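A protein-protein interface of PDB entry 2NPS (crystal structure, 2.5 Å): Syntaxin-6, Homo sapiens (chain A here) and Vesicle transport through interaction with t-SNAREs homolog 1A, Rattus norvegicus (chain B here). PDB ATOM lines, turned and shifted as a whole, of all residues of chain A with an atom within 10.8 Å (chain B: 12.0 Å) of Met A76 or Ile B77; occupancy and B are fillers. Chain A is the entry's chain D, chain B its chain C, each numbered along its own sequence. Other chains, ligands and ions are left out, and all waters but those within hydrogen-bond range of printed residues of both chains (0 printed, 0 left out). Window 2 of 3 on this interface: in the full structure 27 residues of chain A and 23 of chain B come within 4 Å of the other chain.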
ATOM      1  N   LYS A  68      27.243  -2.627   8.664  1.00  0.00           N
ATOM      2  CA  LYS A  68      28.588  -2.752   9.209  1.00  0.00           C
ATOM      3  C   LYS A  68      28.705  -1.844  10.440  1.00  0.00           C
ATOM      4  O   LYS A  68      29.247  -2.240  11.462  1.00  0.00           O
ATOM      5  CB  LYS A  68      29.640  -2.383   8.155  1.00  0.00           C
ATOM      6  N   LYS A  69      28.184  -0.627  10.338  1.00  0.00           N
ATOM      7  CA  LYS A  69      28.203   0.313  11.457  1.00  0.00           C
ATOM      8  C   LYS A  69      27.544  -0.366  12.650  1.00  0.00           C
ATOM      9  O   LYS A  69      27.997  -0.241  13.786  1.00  0.00           O
ATOM     10  CB  LYS A  69      27.377   1.549  11.118  1.00  0.00           C
ATOM     11  CG  LYS A  69      28.124   2.842  10.905  1.00  0.00           C
ATOM     12  CD  LYS A  69      27.137   3.901  10.400  1.00  0.00           C
ATOM     13  CE  LYS A  69      27.796   5.264  10.206  1.00  0.00           C
ATOM     14  NZ  LYS A  69      28.315   5.772  11.502  1.00  0.00           N
ATOM     15  N   LEU A  70      26.453  -1.072  12.360  1.00  0.00           N
ATOM     16  CA  LEU A  70      25.658  -1.768  13.357  1.00  0.00           C
ATOM     17  C   LEU A  70      26.461  -2.856  14.027  1.00  0.00           C
ATOM     18  O   LEU A  70      26.640  -2.852  15.244  1.00  0.00           O
ATOM     19  CB  LEU A  70      24.426  -2.378  12.695  1.00  0.00           C
ATOM     20  CG  LEU A  70      23.132  -2.493  13.508  1.00  0.00           C
ATOM     21  CD1 LEU A  70      22.100  -3.215  12.654  1.00  0.00           C
ATOM     22  CD2 LEU A  70      23.343  -3.252  14.802  1.00  0.00           C
ATOM     23  N   ALA A  71      26.942  -3.792  13.219  1.00  0.00           N
ATOM     24  CA  ALA A  71      27.750  -4.888  13.721  1.00  0.00           C
ATOM     25  C   ALA A  71      28.875  -4.325  14.581  1.00  0.00           C
ATOM     26  O   ALA A  71      29.249  -4.924  15.582  1.00  0.00           O
ATOM     27  CB  ALA A  71      28.316  -5.686  12.567  1.00  0.00           C
ATOM     28  N   LYS A  72      29.407  -3.172  14.188  1.00  0.00           N
ATOM     29  CA  LYS A  72      30.485  -2.535  14.940  1.00  0.00           C
ATOM     30  C   LYS A  72      30.027  -2.066  16.315  1.00  0.00           C
ATOM     31  O   LYS A  72      30.692  -2.321  17.315  1.00  0.00           O
ATOM     32  CB  LYS A  72      31.059  -1.349  14.165  1.00  0.00           C
ATOM     33  CG  LYS A  72      32.053  -0.529  14.965  1.00  0.00           C
ATOM     34  N   VAL A  73      28.899  -1.363  16.356  1.00  0.00           N
ATOM     35  CA  VAL A  73      28.348  -0.893  17.618  1.00  0.00           C
ATOM     36  C   VAL A  73      27.997  -2.085  18.486  1.00  0.00           C
ATOM     37  O   VAL A  73      28.210  -2.066  19.689  1.00  0.00           O
ATOM     38  CB  VAL A  73      27.068  -0.091  17.413  1.00  0.00           C
ATOM     39  CG1 VAL A  73      26.476   0.288  18.761  1.00  0.00           C
ATOM     40  CG2 VAL A  73      27.356   1.129  16.581  1.00  0.00           C
ATOM     41  N   SER A  74      27.448  -3.124  17.872  1.00  0.00           N
ATOM     42  CA  SER A  74      27.070  -4.312  18.621  1.00  0.00           C
ATOM     43  C   SER A  74      28.259  -4.903  19.359  1.00  0.00           C
ATOM     44  O   SER A  74      28.083  -5.615  20.350  1.00  0.00           O
ATOM     45  CB  SER A  74      26.481  -5.365  17.693  1.00  0.00           C
ATOM     46  OG  SER A  74      26.311  -6.584  18.392  1.00  0.00           O
ATOM     47  N   HIS A  75      29.465  -4.610  18.881  1.00  0.00           N
ATOM     48  CA  HIS A  75      30.681  -5.115  19.507  1.00  0.00           C
ATOM     49  C   HIS A  75      31.248  -4.104  20.485  1.00  0.00           C
ATOM     50  O   HIS A  75      31.586  -4.433  21.616  1.00  0.00           O
ATOM     51  CB  HIS A  75      31.719  -5.439  18.436  1.00  0.00           C
ATOM     52  CG  HIS A  75      31.563  -6.804  17.839  1.00  0.00           C
ATOM     53  ND1 HIS A  75      30.371  -7.262  17.319  1.00  0.00           N
ATOM     54  CD2 HIS A  75      32.454  -7.812  17.683  1.00  0.00           C
ATOM     55  CE1 HIS A  75      30.535  -8.494  16.868  1.00  0.00           C
ATOM     56  NE2 HIS A  75      31.790  -8.851  17.077  1.00  0.00           N
ATOM     57  N   MET A  76      31.349  -2.866  20.029  1.00  0.00           N
ATOM     58  CA  MET A  76      31.867  -1.768  20.834  1.00  0.00           C
ATOM     59  C   MET A  76      31.309  -1.691  22.259  1.00  0.00           C
ATOM     60  O   MET A  76      31.908  -1.057  23.136  1.00  0.00           O
ATOM     61  CB  MET A  76      31.586  -0.455  20.116  1.00  0.00           C
ATOM     62  CG  MET A  76      32.531  -0.150  18.992  1.00  0.00           C
ATOM     63  SD  MET A  76      33.743   1.023  19.570  1.00  0.00           S
ATOM     64  CE  MET A  76      32.746   2.520  19.537  1.00  0.00           C
ATOM     65  N   THR A  77      30.160  -2.323  22.483  1.00  0.00           N
ATOM     66  CA  THR A  77      29.531  -2.319  23.797  1.00  0.00           C
ATOM     67  C   THR A  77      29.447  -3.704  24.422  1.00  0.00           C
ATOM     68  O   THR A  77      30.103  -3.966  25.422  1.00  0.00           O
ATOM     69  CB  THR A  77      28.118  -1.718  23.736  1.00  0.00           C
ATOM     70  OG1 THR A  77      27.410  -2.275  22.625  1.00  0.00           O
ATOM     71  CG2 THR A  77      28.188  -0.204  23.582  1.00  0.00           C
ATOM     72  N   SER A  78      28.648  -4.592  23.842  1.00  0.00           N
ATOM     73  CA  SER A  78      28.514  -5.939  24.392  1.00  0.00           C
ATOM     74  C   SER A  78      29.705  -6.810  24.015  1.00  0.00           C
ATOM     75  O   SER A  78      29.553  -7.910  23.486  1.00  0.00           O
ATOM     76  N   ASP A  79      30.895  -6.295  24.290  1.00  0.00           N
ATOM     77  CA  ASP A  79      32.139  -6.995  24.005  1.00  0.00           C
ATOM     78  C   ASP A  79      33.221  -6.140  24.657  1.00  0.00           C
ATOM     79  O   ASP A  79      34.403  -6.223  24.329  1.00  0.00           O
ATOM     80  CB  ASP A  79      32.332  -7.094  22.486  1.00  0.00           C
ATOM     81  CG  ASP A  79      33.496  -7.978  22.095  1.00  0.00           C
ATOM     82  OD1 ASP A  79      34.565  -7.435  21.739  1.00  0.00           O
ATOM     83  OD2 ASP A  79      33.340  -9.215  22.144  1.00  0.00           O
ATOM     84  N   ARG A  80      32.772  -5.313  25.595  1.00  0.00           N
ATOM     85  CA  ARG A  80      33.630  -4.402  26.338  1.00  0.00           C
ATOM     86  C   ARG A  80      33.143  -4.385  27.787  1.00  0.00           C
ATOM     87  O   ARG A  80      31.981  -3.995  28.036  1.00  0.00           O
ATOM     88  N   ARG B  68      23.012   7.983  10.780  1.00  0.00           N
ATOM     89  CA  ARG B  68      23.269   9.030  11.750  1.00  0.00           C
ATOM     90  C   ARG B  68      23.106   8.454  13.173  1.00  0.00           C
ATOM     91  O   ARG B  68      23.987   8.630  14.008  1.00  0.00           O
ATOM     92  CB  ARG B  68      22.339  10.225  11.494  1.00  0.00           C
ATOM     93  CG  ARG B  68      22.123  11.154  12.679  1.00  0.00           C
ATOM     94  CD  ARG B  68      21.782  12.597  12.254  1.00  0.00           C
ATOM     95  NE  ARG B  68      22.979  13.449  12.179  1.00  0.00           N
ATOM     96  CZ  ARG B  68      23.598  13.806  11.052  1.00  0.00           C
ATOM     97  NH1 ARG B  68      24.681  14.576  11.094  1.00  0.00           N
ATOM     98  NH2 ARG B  68      23.129  13.416   9.872  1.00  0.00           N
ATOM     99  N   ILE B  69      22.017   7.729  13.443  1.00  0.00           N
ATOM    100  CA  ILE B  69      21.797   7.164  14.785  1.00  0.00           C
ATOM    101  C   ILE B  69      22.948   6.278  15.223  1.00  0.00           C
ATOM    102  O   ILE B  69      23.383   6.339  16.368  1.00  0.00           O
ATOM    103  CB  ILE B  69      20.479   6.331  14.875  1.00  0.00           C
ATOM    104  CG1 ILE B  69      19.276   7.227  14.676  1.00  0.00           C
ATOM    105  CG2 ILE B  69      20.340   5.677  16.238  1.00  0.00           C
ATOM    106  CD1 ILE B  69      17.983   6.495  14.730  1.00  0.00           C
ATOM    107  N   LEU B  70      23.450   5.464  14.303  1.00  0.00           N
ATOM    108  CA  LEU B  70      24.546   4.551  14.616  1.00  0.00           C
ATOM    109  C   LEU B  70      25.832   5.268  14.944  1.00  0.00           C
ATOM    110  O   LEU B  70      26.572   4.865  15.833  1.00  0.00           O
ATOM    111  CB  LEU B  70      24.779   3.590  13.464  1.00  0.00           C
ATOM    112  CG  LEU B  70      23.766   2.455  13.430  1.00  0.00           C
ATOM    113  CD1 LEU B  70      24.090   1.540  12.282  1.00  0.00           C
ATOM    114  CD2 LEU B  70      23.780   1.691  14.759  1.00  0.00           C
ATOM    115  N   THR B  71      26.096   6.332  14.199  1.00  0.00           N
ATOM    116  CA  THR B  71      27.272   7.148  14.425  1.00  0.00           C
ATOM    117  C   THR B  71      27.177   7.646  15.861  1.00  0.00           C
ATOM    118  O   THR B  71      28.121   7.532  16.645  1.00  0.00           O
ATOM    119  CB  THR B  71      27.285   8.389  13.502  1.00  0.00           C
ATOM    120  OG1 THR B  71      27.449   7.987  12.137  1.00  0.00           O
ATOM    121  CG2 THR B  71      28.402   9.310  13.893  1.00  0.00           C
ATOM    122  N   GLY B  72      26.013   8.212  16.180  1.00  0.00           N
ATOM    123  CA  GLY B  72      25.754   8.749  17.501  1.00  0.00           C
ATOM    124  C   GLY B  72      25.969   7.722  18.583  1.00  0.00           C
ATOM    125  O   GLY B  72      26.471   8.048  19.652  1.00  0.00           O
ATOM    126  N   MET B  73      25.594   6.474  18.318  1.00  0.00           N
ATOM    127  CA  MET B  73      25.773   5.420  19.307  1.00  0.00           C
ATOM    128  C   MET B  73      27.249   5.113  19.435  1.00  0.00           C
ATOM    129  O   MET B  73      27.746   4.935  20.544  1.00  0.00           O
ATOM    130  CB  MET B  73      24.999   4.153  18.910  1.00  0.00           C
ATOM    131  CG  MET B  73      23.477   4.266  19.071  1.00  0.00           C
ATOM    132  SD  MET B  73      22.621   2.728  18.738  1.00  0.00           S
ATOM    133  CE  MET B  73      22.955   1.856  20.174  1.00  0.00           C
ATOM    134  N   LEU B  74      27.936   5.062  18.293  1.00  0.00           N
ATOM    135  CA  LEU B  74      29.379   4.803  18.233  1.00  0.00           C
ATOM    136  C   LEU B  74      30.142   5.820  19.069  1.00  0.00           C
ATOM    137  O   LEU B  74      31.214   5.528  19.598  1.00  0.00           O
ATOM    138  CB  LEU B  74      29.892   4.884  16.791  1.00  0.00           C
ATOM    139  CG  LEU B  74      29.689   3.650  15.922  1.00  0.00           C
ATOM    140  CD1 LEU B  74      30.038   3.944  14.474  1.00  0.00           C
ATOM    141  CD2 LEU B  74      30.558   2.528  16.459  1.00  0.00           C
ATOM    142  N   ARG B  75      29.594   7.024  19.166  1.00  0.00           N
ATOM    143  CA  ARG B  75      30.233   8.068  19.940  1.00  0.00           C
ATOM    144  C   ARG B  75      30.094   7.746  21.416  1.00  0.00           C
ATOM    145  O   ARG B  75      31.087   7.559  22.108  1.00  0.00           O
ATOM    146  CB  ARG B  75      29.604   9.425  19.623  1.00  0.00           C
ATOM    147  CG  ARG B  75      30.566  10.573  19.812  1.00  0.00           C
ATOM    148  CD  ARG B  75      30.007  11.869  19.278  1.00  0.00           C
ATOM    149  NE  ARG B  75      29.812  11.833  17.835  1.00  0.00           N
ATOM    150  CZ  ARG B  75      29.229  12.807  17.146  1.00  0.00           C
ATOM    151  NH1 ARG B  75      29.087  12.698  15.834  1.00  0.00           N
ATOM    152  NH2 ARG B  75      28.788  13.894  17.774  1.00  0.00           N
ATOM    153  N   ARG B  76      28.858   7.649  21.892  1.00  0.00           N
ATOM    154  CA  ARG B  76      28.612   7.351  23.298  1.00  0.00           C
ATOM    155  C   ARG B  76      29.201   6.026  23.802  1.00  0.00           C
ATOM    156  O   ARG B  76      29.180   5.747  24.996  1.00  0.00           O
ATOM    157  CB  ARG B  76      27.112   7.417  23.578  1.00  0.00           C
ATOM    158  N   ILE B  77      29.744   5.218  22.899  1.00  0.00           N
ATOM    159  CA  ILE B  77      30.359   3.955  23.305  1.00  0.00           C
ATOM    160  C   ILE B  77      31.755   4.211  23.860  1.00  0.00           C
ATOM    161  O   ILE B  77      32.290   3.420  24.639  1.00  0.00           O
ATOM    162  CB  ILE B  77      30.477   2.967  22.127  1.00  0.00           C
ATOM    163  N   ILE B  78      32.350   5.319  23.430  1.00  0.00           N
ATOM    164  CA  ILE B  78      33.671   5.708  23.904  1.00  0.00           C
ATOM    165  C   ILE B  78      33.428   6.673  25.051  1.00  0.00           C
ATOM    166  O   ILE B  78      34.276   7.497  25.367  1.00  0.00           O
ATOM    167  N   GLN B  79      32.243   6.571  25.650  1.00  0.00           N
ATOM    168  CA  GLN B  79      31.853   7.423  26.771  1.00  0.00           C
ATOM    169  C   GLN B  79      31.919   8.900  26.385  1.00  0.00           C
ATOM    170  O   GLN B  79      32.139   9.185  25.188  1.00  0.00           O
ATOM    171  CB  GLN B  79      32.758   7.147  27.978  1.00  0.00           C
ATOM    172  CG  GLN B  79      33.087   5.669  28.179  1.00  0.00           C
ATOM    173  CD  GLN B  79      31.849   4.780  28.137  1.00  0.00           C
ATOM    174  OE1 GLN B  79      30.731   5.251  27.899  1.00  0.00           O
ATOM    175  NE2 GLN B  79      32.047   3.485  28.365  1.00  0.00           N
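The side-chain amino group (NZ) of Lys A69 is in hydrogen-bond range of the side-chain hydroxyl (OG1) of Thr B71 (2.5 Å).
OG1 of Thr A77 is in hydrogen-bond range of O of Val A73 (3.1 Å).
CD1 of Leu B70 touches CB of Lys A69, 3.5 Å away.
Lys A69 touches Leu B74 (NZ to CD1, 3.9 Å).
CD1 of Leu B70 touches N of Leu A70 (3.5 Å).
CG of Lys A72 touches CD2 of Leu B74 (3.7 Å).
O of Leu B70 touches CG2 of Val A73 (3.9 Å).
CG2 of Val A73 touches CD2 of Leu B74 (3.5 Å).
O of Leu B74 touches CE of Met A76, 3.4 Å away.
CE of Met A76 touches CB of Ile B77, 3.5 Å away.
Of the printed residues of chain B, Lys A72 touches Leu B74 (3.7 Å).
Val A73 touches just these residues of chain B: Leu B70 and Leu B74.
Met A76 touches just these residues of chain B: Leu B74 (3.4 Å) and Ile B77 (3.5 Å).
No residue of chain B comes within 4 Å of Thr A77.
No residue of chain B comes within 4 Å of Ser A78.
No residue of chain B comes within 4 Å of Asp A79.
Of the printed residues of chain A, Leu B70 touches Lys A69, Leu A70 and Val A73.
Printed residues of chain A within 4 Å of Thr B71: Lys A69 (2.5 Å).
Of chain A, only Lys A69 (3.9 Å), Lys A72 (3.7 Å), Val A73 (3.5 Å) and Met A76 (3.4 Å) come within 4 Å of Leu B74.
Of the printed residues of chain A, Ile B77 touches Met A76 (3.5 Å).
No residue of chain A comes within 4 Å of Ile B78.
The nearest residue of chain B that does not touch Met A76 is Ile B78 (4.8 Å).
The nearest residue of chain A that does not touch Ile B77 is Thr A77 (4.2 Å).
Along chain B the printed residues that touch a printed residue of chain A span positions 70 to 77.
Printed residues of chain A that touch a printed residue of chain B: Lys A69, Leu A70, Lys A72, Val A73 and Met A76.
Hydrophobic or aromatic side chains of chain A within 4 Å of the printed part of chain B: Leu A70, Val A73 and Met A76.
Among the printed residues, 9 pairs touch across the chains.
Among the printed residues, no Asp or Glu carboxylate lies within 4 Å of a Lys or Arg side-chain nitrogen of the other chain.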
